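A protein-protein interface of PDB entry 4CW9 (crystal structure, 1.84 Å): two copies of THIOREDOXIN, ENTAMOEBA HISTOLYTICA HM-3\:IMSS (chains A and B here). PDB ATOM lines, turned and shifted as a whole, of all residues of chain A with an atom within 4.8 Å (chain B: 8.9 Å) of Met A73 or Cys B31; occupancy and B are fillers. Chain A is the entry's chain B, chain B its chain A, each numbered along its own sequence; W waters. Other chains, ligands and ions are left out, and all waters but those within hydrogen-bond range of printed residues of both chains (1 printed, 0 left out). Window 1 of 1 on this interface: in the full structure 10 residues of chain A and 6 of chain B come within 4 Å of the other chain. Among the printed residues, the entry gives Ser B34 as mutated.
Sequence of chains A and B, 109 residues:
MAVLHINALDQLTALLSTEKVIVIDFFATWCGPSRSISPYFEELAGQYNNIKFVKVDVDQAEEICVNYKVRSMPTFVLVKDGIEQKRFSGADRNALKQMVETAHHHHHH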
ATOM      1  N   PHE A  26      -8.887  -1.453   3.236  1.00  0.00           N
ATOM      2  CA  PHE A  26      -8.366  -2.804   3.272  1.00  0.00           C
ATOM      3  C   PHE A  26      -9.232  -3.627   4.215  1.00  0.00           C
ATOM      4  O   PHE A  26      -9.206  -3.381   5.452  1.00  0.00           O
ATOM      5  CB  PHE A  26      -6.895  -2.796   3.787  1.00  0.00           C
ATOM      6  CG  PHE A  26      -5.932  -2.227   2.787  1.00  0.00           C
ATOM      7  CD1 PHE A  26      -5.746  -0.882   2.686  1.00  0.00           C
ATOM      8  CD2 PHE A  26      -5.236  -3.074   1.897  1.00  0.00           C
ATOM      9  CE1 PHE A  26      -4.891  -0.333   1.712  1.00  0.00           C
ATOM     10  CE2 PHE A  26      -4.360  -2.544   0.946  1.00  0.00           C
ATOM     11  CZ  PHE A  26      -4.208  -1.169   0.851  1.00  0.00           C
ATOM     12  N   PHE A  27      -9.925  -4.633   3.665  1.00  0.00           N
ATOM     13  CA  PHE A  27     -10.937  -5.363   4.414  1.00  0.00           C
ATOM     14  C   PHE A  27     -10.700  -6.865   4.404  1.00  0.00           C
ATOM     15  O   PHE A  27      -9.917  -7.429   3.641  1.00  0.00           O
ATOM     16  CB  PHE A  27     -12.361  -5.004   3.927  1.00  0.00           C
ATOM     17  CG  PHE A  27     -12.702  -5.624   2.636  1.00  0.00           C
ATOM     18  CD1 PHE A  27     -12.314  -5.026   1.440  1.00  0.00           C
ATOM     19  CD2 PHE A  27     -13.354  -6.836   2.600  1.00  0.00           C
ATOM     20  CE1 PHE A  27     -12.578  -5.640   0.228  1.00  0.00           C
ATOM     21  CE2 PHE A  27     -13.625  -7.458   1.408  1.00  0.00           C
ATOM     22  CZ  PHE A  27     -13.254  -6.853   0.202  1.00  0.00           C
ATOM     23  N   ALA A  28     -11.365  -7.514   5.353  1.00  0.00           N
ATOM     24  CA  ALA A  28     -11.437  -8.954   5.404  1.00  0.00           C
ATOM     25  C   ALA A  28     -12.863  -9.234   5.818  1.00  0.00           C
ATOM     26  O   ALA A  28     -13.374  -8.596   6.732  1.00  0.00           O
ATOM     27  CB  ALA A  28     -10.502  -9.486   6.428  1.00  0.00           C
ATOM     28  N   TRP A  30     -14.053 -12.090   6.956  1.00  0.00           N
ATOM     29  CA  TRP A  30     -13.856 -12.753   8.232  1.00  0.00           C
ATOM     30  C   TRP A  30     -13.428 -11.868   9.418  1.00  0.00           C
ATOM     31  O   TRP A  30     -13.167 -12.387  10.491  1.00  0.00           O
ATOM     32  CB  TRP A  30     -12.829 -13.855   8.058  1.00  0.00           C
ATOM     33  CG  TRP A  30     -11.418 -13.444   7.576  1.00  0.00           C
ATOM     34  CD1 TRP A  30     -10.891 -13.671   6.328  1.00  0.00           C
ATOM     35  CD2 TRP A  30     -10.353 -12.840   8.347  1.00  0.00           C
ATOM     36  NE1 TRP A  30      -9.599 -13.222   6.264  1.00  0.00           N
ATOM     37  CE2 TRP A  30      -9.238 -12.714   7.485  1.00  0.00           C
ATOM     38  CE3 TRP A  30     -10.233 -12.384   9.671  1.00  0.00           C
ATOM     39  CZ2 TRP A  30      -8.016 -12.149   7.901  1.00  0.00           C
ATOM     40  CZ3 TRP A  30      -8.996 -11.827  10.090  1.00  0.00           C
ATOM     41  CH2 TRP A  30      -7.915 -11.706   9.186  1.00  0.00           C
ATOM     42  N   CYS A  31     -13.355 -10.556   9.250  1.00  0.00           N
ATOM     43  CA  CYS A  31     -13.021  -9.678  10.361  1.00  0.00           C
ATOM     44  C   CYS A  31     -14.219  -8.832  10.771  1.00  0.00           C
ATOM     45  O   CYS A  31     -14.653  -7.939  10.031  1.00  0.00           O
ATOM     46  CB  CYS A  31     -11.795  -8.808  10.034  1.00  0.00           C
ATOM     47  SG  CYS A  31     -11.357  -7.623  11.318  1.00  0.00           S
ATOM     48  N   GLY A  32     -14.715  -9.114  11.996  1.00  0.00           N
ATOM     49  CA  GLY A  32     -15.860  -8.432  12.567  1.00  0.00           C
ATOM     50  C   GLY A  32     -15.850  -6.950  12.475  1.00  0.00           C
ATOM     51  O   GLY A  32     -16.761  -6.333  11.867  1.00  0.00           O
ATOM     52  N   PRO A  33     -14.812  -6.311  13.054  1.00  0.00           N
ATOM     53  CA  PRO A  33     -14.793  -4.860  12.861  1.00  0.00           C
ATOM     54  C   PRO A  33     -14.760  -4.383  11.388  1.00  0.00           C
ATOM     55  O   PRO A  33     -15.289  -3.327  11.097  1.00  0.00           O
ATOM     56  CB  PRO A  33     -13.571  -4.378  13.676  1.00  0.00           C
ATOM     57  CG  PRO A  33     -12.790  -5.626  13.998  1.00  0.00           C
ATOM     58  CD  PRO A  33     -13.744  -6.784  13.953  1.00  0.00           C
ATOM     59  N   VAL A  58      -7.845  -8.285   1.465  1.00  0.00           N
ATOM     60  CA  VAL A  58      -6.510  -8.676   1.855  1.00  0.00           C
ATOM     61  C   VAL A  58      -6.221 -10.155   1.562  1.00  0.00           C
ATOM     62  O   VAL A  58      -5.089 -10.533   1.276  1.00  0.00           O
ATOM     63  CB  VAL A  58      -6.265  -8.364   3.350  1.00  0.00           C
ATOM     64  CG1 VAL A  58      -6.510  -6.883   3.664  1.00  0.00           C
ATOM     65  CG2 VAL A  58      -7.125  -9.251   4.230  1.00  0.00           C
ATOM     66  N   VAL A  70       0.222  -3.458   4.946  1.00  0.00           N
ATOM     67  CA  VAL A  70      -1.055  -3.652   5.616  1.00  0.00           C
ATOM     68  C   VAL A  70      -1.004  -4.992   6.243  1.00  0.00           C
ATOM     69  O   VAL A  70      -0.819  -5.952   5.557  1.00  0.00           O
ATOM     70  CB  VAL A  70      -2.273  -3.518   4.704  1.00  0.00           C
ATOM     71  CG1 VAL A  70      -3.527  -4.013   5.462  1.00  0.00           C
ATOM     72  CG2 VAL A  70      -2.439  -2.069   4.313  1.00  0.00           C
ATOM     73  N   ARG A  71      -1.079  -5.029   7.581  1.00  0.00           N
ATOM     74  CA  ARG A  71      -1.183  -6.272   8.363  1.00  0.00           C
ATOM     75  C   ARG A  71      -2.399  -6.305   9.306  1.00  0.00           C
ATOM     76  O   ARG A  71      -2.496  -7.195  10.160  1.00  0.00           O
ATOM     77  CB  ARG A  71       0.083  -6.484   9.200  1.00  0.00           C
ATOM     78  CG  ARG A  71       1.374  -6.282   8.453  1.00  0.00           C
ATOM     79  CD  ARG A  71       2.573  -6.847   9.222  1.00  0.00           C
ATOM     80  NE  ARG A  71       3.842  -6.656   8.513  1.00  0.00           N
ATOM     81  CZ  ARG A  71       4.456  -5.475   8.340  1.00  0.00           C
ATOM     82  NH1 ARG A  71       3.937  -4.342   8.797  1.00  0.00           N
ATOM     83  NH2 ARG A  71       5.610  -5.427   7.665  1.00  0.00           N
ATOM     84  N   SER A  72      -3.325  -5.365   9.151  1.00  0.00           N
ATOM     85  CA  SER A  72      -4.453  -5.322  10.051  1.00  0.00           C
ATOM     86  C   SER A  72      -5.584  -4.706   9.315  1.00  0.00           C
ATOM     87  O   SER A  72      -5.390  -3.894   8.385  1.00  0.00           O
ATOM     88  CB  SER A  72      -4.155  -4.475  11.260  1.00  0.00           C
ATOM     89  OG  SER A  72      -4.000  -3.103  10.863  1.00  0.00           O
ATOM     90  N   MET A  73      -6.777  -5.134   9.703  1.00  0.00           N
ATOM     91  CA  MET A  73      -7.972  -4.614   9.104  1.00  0.00           C
ATOM     92  C   MET A  73      -9.127  -4.412  10.089  1.00  0.00           C
ATOM     93  O   MET A  73      -9.261  -5.126  11.056  1.00  0.00           O
ATOM     94  CB  MET A  73      -8.396  -5.402   7.869  1.00  0.00           C
ATOM     95  CG  MET A  73      -7.872  -6.792   7.662  1.00  0.00           C
ATOM     96  SD  MET A  73      -6.113  -7.207   7.458  1.00  0.00           S
ATOM     97  CE  MET A  73      -6.406  -8.892   7.951  1.00  0.00           C
ATOM     98  N   PRO A  74      -9.956  -3.416   9.817  1.00  0.00           N
ATOM     99  CA  PRO A  74      -9.858  -2.589   8.620  1.00  0.00           C
ATOM    100  C   PRO A  74      -8.776  -1.513   8.706  1.00  0.00           C
ATOM    101  O   PRO A  74      -8.602  -0.926   9.766  1.00  0.00           O
ATOM    102  CB  PRO A  74     -11.233  -1.918   8.547  1.00  0.00           C
ATOM    103  CG  PRO A  74     -11.715  -1.904   9.960  1.00  0.00           C
ATOM    104  CD  PRO A  74     -11.197  -3.156  10.579  1.00  0.00           C
ATOM    105  N   THR A  75      -8.089  -1.238   7.573  1.00  0.00           N
ATOM    106  CA  THR A  75      -7.099  -0.145   7.509  1.00  0.00           C
ATOM    107  C   THR A  75      -7.505   0.761   6.413  1.00  0.00           C
ATOM    108  O   THR A  75      -7.744   0.306   5.316  1.00  0.00           O
ATOM    109  CB  THR A  75      -5.675  -0.685   7.240  1.00  0.00           C
ATOM    110  OG1 THR A  75      -5.249  -1.556   8.313  1.00  0.00           O
ATOM    111  CG2 THR A  75      -4.641   0.428   7.014  1.00  0.00           C
ATOM    112  N   PHE B  27      -7.612  -5.848  23.632  1.00  0.00           N
ATOM    113  CA  PHE B  27      -8.059  -6.059  22.278  1.00  0.00           C
ATOM    114  C   PHE B  27      -8.020  -4.745  21.490  1.00  0.00           C
ATOM    115  O   PHE B  27      -7.780  -3.670  22.037  1.00  0.00           O
ATOM    116  CB  PHE B  27      -9.476  -6.644  22.312  1.00  0.00           C
ATOM    117  CG  PHE B  27     -10.527  -5.611  22.510  1.00  0.00           C
ATOM    118  CD1 PHE B  27     -10.758  -5.086  23.773  1.00  0.00           C
ATOM    119  CD2 PHE B  27     -11.317  -5.217  21.477  1.00  0.00           C
ATOM    120  CE1 PHE B  27     -11.720  -4.134  23.965  1.00  0.00           C
ATOM    121  CE2 PHE B  27     -12.275  -4.265  21.652  1.00  0.00           C
ATOM    122  CZ  PHE B  27     -12.493  -3.723  22.912  1.00  0.00           C
ATOM    123  N   ALA B  28      -8.237  -4.853  20.189  1.00  0.00           N
ATOM    124  CA  ALA B  28      -8.337  -3.678  19.283  1.00  0.00           C
ATOM    125  C   ALA B  28      -9.580  -3.824  18.426  1.00  0.00           C
ATOM    126  O   ALA B  28     -10.047  -4.931  18.265  1.00  0.00           O
ATOM    127  CB  ALA B  28      -7.122  -3.584  18.378  1.00  0.00           C
ATOM    128  N   THR B  29     -10.066  -2.707  17.881  1.00  0.00           N
ATOM    129  CA  THR B  29     -11.186  -2.631  16.924  1.00  0.00           C
ATOM    130  C   THR B  29     -10.745  -2.931  15.443  1.00  0.00           C
ATOM    131  O   THR B  29     -11.315  -2.418  14.484  1.00  0.00           O
ATOM    132  CB  THR B  29     -11.769  -1.217  16.955  1.00  0.00           C
ATOM    133  OG1 THR B  29     -10.738  -0.240  16.760  1.00  0.00           O
ATOM    134  CG2 THR B  29     -12.465  -0.888  18.307  1.00  0.00           C
ATOM    135  N   TRP B  30      -9.721  -3.757  15.308  1.00  0.00           N
ATOM    136  CA  TRP B  30      -9.188  -4.235  14.055  1.00  0.00           C
ATOM    137  C   TRP B  30      -8.700  -5.615  14.359  1.00  0.00           C
ATOM    138  O   TRP B  30      -8.444  -5.926  15.517  1.00  0.00           O
ATOM    139  CB  TRP B  30      -8.037  -3.322  13.538  1.00  0.00           C
ATOM    140  CG  TRP B  30      -6.949  -2.904  14.506  1.00  0.00           C
ATOM    141  CD1 TRP B  30      -6.845  -1.709  15.129  1.00  0.00           C
ATOM    142  CD2 TRP B  30      -5.777  -3.654  14.885  1.00  0.00           C
ATOM    143  NE1 TRP B  30      -5.685  -1.676  15.900  1.00  0.00           N
ATOM    144  CE2 TRP B  30      -5.045  -2.878  15.770  1.00  0.00           C
ATOM    145  CE3 TRP B  30      -5.296  -4.932  14.573  1.00  0.00           C
ATOM    146  CZ2 TRP B  30      -3.828  -3.322  16.320  1.00  0.00           C
ATOM    147  CZ3 TRP B  30      -4.096  -5.388  15.147  1.00  0.00           C
ATOM    148  CH2 TRP B  30      -3.394  -4.594  16.013  1.00  0.00           C
ATOM    149  N   CYS B  31      -8.585  -6.441  13.330  1.00  0.00           N
ATOM    150  CA  CYS B  31      -7.978  -7.751  13.391  1.00  0.00           C
ATOM    151  C   CYS B  31      -6.636  -7.759  12.706  1.00  0.00           C
ATOM    152  O   CYS B  31      -6.386  -6.937  11.811  1.00  0.00           O
ATOM    153  CB  CYS B  31      -8.795  -8.789  12.622  1.00  0.00           C
ATOM    154  SG  CYS B  31     -10.585  -8.736  12.906  1.00  0.00           S
ATOM    155  N   GLY B  32      -5.816  -8.739  13.101  1.00  0.00           N
ATOM    156  CA  GLY B  32      -4.535  -9.034  12.519  1.00  0.00           C
ATOM    157  C   GLY B  32      -4.587 -10.277  11.676  1.00  0.00           C
ATOM    158  O   GLY B  32      -5.369 -10.323  10.756  1.00  0.00           O
ATOM    159  N   PRO B  33      -3.783 -11.298  11.989  1.00  0.00           N
ATOM    160  CA  PRO B  33      -3.740 -12.570  11.236  1.00  0.00           C
ATOM    161  C   PRO B  33      -4.986 -13.519  11.293  1.00  0.00           C
ATOM    162  O   PRO B  33      -5.131 -14.415  10.441  1.00  0.00           O
ATOM    163  CB  PRO B  33      -2.554 -13.290  11.872  1.00  0.00           C
ATOM    164  CG  PRO B  33      -2.546 -12.785  13.289  1.00  0.00           C
ATOM    165  CD  PRO B  33      -2.878 -11.332  13.149  1.00  0.00           C
ATOM    166  N   SER B  34      -5.837 -13.357  12.307  1.00  0.00           N
ATOM    167  CA  SER B  34      -6.975 -14.230  12.464  1.00  0.00           C
ATOM    168  C   SER B  34      -8.191 -13.485  12.963  1.00  0.00           C
ATOM    169  O   SER B  34      -8.140 -12.323  13.392  1.00  0.00           O
ATOM    170  CB  SER B  34      -6.625 -15.408  13.358  1.00  0.00           C
ATOM    171  OG  SER B  34      -5.822 -14.990  14.448  1.00  0.00           O
ATOM    172  N   ARG B  35      -9.325 -14.157  12.868  1.00  0.00           N
ATOM    173  CA  ARG B  35     -10.559 -13.518  13.285  1.00  0.00           C
ATOM    174  C   ARG B  35     -10.464 -13.259  14.789  1.00  0.00           C
ATOM    175  O   ARG B  35      -9.730 -13.925  15.540  1.00  0.00           O
ATOM    176  CB  ARG B  35     -11.799 -14.389  12.965  1.00  0.00           C
ATOM    177  CG  ARG B  35     -11.711 -15.826  13.434  1.00  0.00           C
ATOM    178  CD  ARG B  35     -13.119 -16.396  13.695  1.00  0.00           C
ATOM    179  N   SER B  36     -11.227 -12.281  15.191  1.00  0.00           N
ATOM    180  CA  SER B  36     -11.494 -12.038  16.565  1.00  0.00           C
ATOM    181  C   SER B  36     -12.043 -13.270  17.337  1.00  0.00           C
ATOM    182  O   SER B  36     -12.897 -13.973  16.865  1.00  0.00           O
ATOM    183  CB  SER B  36     -12.508 -10.880  16.656  1.00  0.00           C
ATOM    184  OG  SER B  36     -12.741 -10.524  17.990  1.00  0.00           O
ATOM    185  N   ILE B  37     -11.547 -13.430  18.546  1.00  0.00           N
ATOM    186  CA  ILE B  37     -11.973 -14.406  19.560  1.00  0.00           C
ATOM    187  C   ILE B  37     -12.980 -13.752  20.584  1.00  0.00           C
ATOM    188  O   ILE B  37     -13.445 -14.375  21.557  1.00  0.00           O
ATOM    189  CB  ILE B  37     -10.651 -14.868  20.196  1.00  0.00           C
ATOM    190  CG1 ILE B  37     -10.672 -16.203  20.848  1.00  0.00           C
ATOM    191  CG2 ILE B  37     -10.100 -13.882  21.192  1.00  0.00           C
ATOM    192  CD1 ILE B  37      -9.337 -16.464  21.538  1.00  0.00           C
ATOM    193  N   SER B  38     -13.334 -12.497  20.361  1.00  0.00           N
ATOM    194  CA  SER B  38     -14.237 -11.754  21.245  1.00  0.00           C
ATOM    195  C   SER B  38     -15.568 -12.455  21.523  1.00  0.00           C
ATOM    196  O   SER B  38     -16.041 -12.376  22.669  1.00  0.00           O
ATOM    197  CB  SER B  38     -14.563 -10.367  20.681  1.00  0.00           C
ATOM    198  OG  SER B  38     -13.409  -9.536  20.816  1.00  0.00           O
ATOM    199  N   MET B  73      -1.893  -7.692  20.002  1.00  0.00           N
ATOM    200  CA  MET B  73      -3.312  -7.840  20.323  1.00  0.00           C
ATOM    201  C   MET B  73      -3.899  -8.974  19.525  1.00  0.00           C
ATOM    202  O   MET B  73      -3.660  -9.047  18.319  1.00  0.00           O
ATOM    203  CB  MET B  73      -4.058  -6.513  20.157  1.00  0.00           C
ATOM    204  CG  MET B  73      -5.025  -6.363  19.016  1.00  0.00           C
ATOM    205  SD  MET B  73      -6.523  -7.366  19.031  1.00  0.00           S
ATOM    206  CE  MET B  73      -6.354  -7.793  17.305  1.00  0.00           C
ATOM    207  N   PRO B  74      -4.643  -9.879  20.208  1.00  0.00           N
ATOM    208  CA  PRO B  74      -5.066  -9.685  21.605  1.00  0.00           C
ATOM    209  C   PRO B  74      -4.051 -10.196  22.576  1.00  0.00           C
ATOM    210  O   PRO B  74      -3.366 -11.186  22.296  1.00  0.00           O
ATOM    211  CB  PRO B  74      -6.340 -10.490  21.706  1.00  0.00           C
ATOM    212  CG  PRO B  74      -6.099 -11.613  20.722  1.00  0.00           C
ATOM    213  CD  PRO B  74      -5.409 -10.957  19.555  1.00  0.00           C
ATOM    214  N   ALA B  91      -5.073 -14.709  19.169  1.00  0.00           N
ATOM    215  CA  ALA B  91      -6.507 -14.992  19.067  1.00  0.00           C
ATOM    216  C   ALA B  91      -6.683 -16.470  18.986  1.00  0.00           C
ATOM    217  O   ALA B  91      -7.149 -16.985  17.966  1.00  0.00           O
ATOM    218  CB  ALA B  91      -7.084 -14.323  17.810  1.00  0.00           C
HETATM  219  O   HOH W   1     -13.564 -11.128  13.632  1.00  0.00           O
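The side-chain sulfur (SG) of Cys A31 forms a disulfide with the side-chain sulfur (SG) of Cys B31.
The backbone NH (N) of Cys B31 is in hydrogen-bond range of the backbone carbonyl oxygen (O) of Met A73, at 2.7 Å.
The side-chain hydroxyl (OG) of Ser A72 sits at hydrogen-bond distance from the side-chain hydroxyl (OG1) of Thr A75 (3.2 Å).
Among the printed residues, merely in contact across the chains: Trp A30 with Cys B31 (3.96 Å), Trp A30 with Gly B32 (3.3 Å), Trp A30 with Ser B34 (3.4 Å), Trp A30 with Arg B35 (3.5 Å), Pro A33 with Thr B29 (3.1 Å), Pro A33 with Trp B30 (3.8 Å), Pro A33 with Cys B31 (3.9 Å), Arg A71 with Gly B32 (3.6 Å), Ser A72 with Trp B30 (3.5 Å), Ser A72 with Cys B31 (3.1 Å), Met A73 with Trp B30 (3.1 Å), Met A73 with Gly B32 (3.3 Å) and Pro A74 with Thr B29 (3.98 Å).
Of the printed residues of chain B, Met A73 touches Trp B30, Cys B31 and Gly B32.
Cys B31 touches five residues of chain A.
Of chain B, only Trp B30 (3.5 Å) and Cys B31 (3.1 Å) come within 4 Å of Ser A72.
Of chain B, only Thr B29 comes within 4 Å of Pro A74.
Of the printed residues of chain A, Thr B29 touches Pro A33 and Pro A74.
Of the printed residues of chain A, Arg B35 touches Trp A30.
The nearest residue of chain B that does not touch Met A73 is Thr B29 (4.8 Å).
The nearest printed residue of chain A that does not touch Cys B31 is Arg A71 (4.2 Å).
The nearest printed residue of chain A that does not touch Thr B29 is Met A73 (4.8 Å).
Of the 15 printed residues of chain B, 6 touch a printed residue of chain A.
Hydrophobic or aromatic side chains of chain B within 4 Å of the printed part of chain A: Trp B30.
Printed residues of chain A that touch a printed residue of chain B: Trp A30, Cys A31, Pro A33, Arg A71, Ser A72, Met A73 and Pro A74.
Among the printed residues, 15 pairs touch across the chains.
Among the printed residues, no Asp or Glu carboxylate lies within 4 Å of a Lys or Arg side-chain nitrogen of the other chain.
Trp A30 touches Cys B31, but with the chains exchanged Cys A31 does not touch Trp B30 (4.5 Å).
Trp A30 touches Gly B32, but with the chains exchanged Gly A32 does not touch Trp B30 (7.3 Å).
Pro A33 touches Trp B30, but with the chains exchanged Trp A30 does not touch Pro B33 (4.04 Å).
Met A73 touches Gly B32, but with the chains exchanged Gly A32 does not touch Met B73 (10.0 Å).
Positions printed for both chains: 27, 28, 30, 31, 32, 33, 73 and 74.
Of the 15 pairs that touch across the chains among the printed residues, 1 has its exchanged pair printed and touching as well.
Water W1 lies within hydrogen-bond range of N of Gly A32, N of Ser B36 and O of Trp A30.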
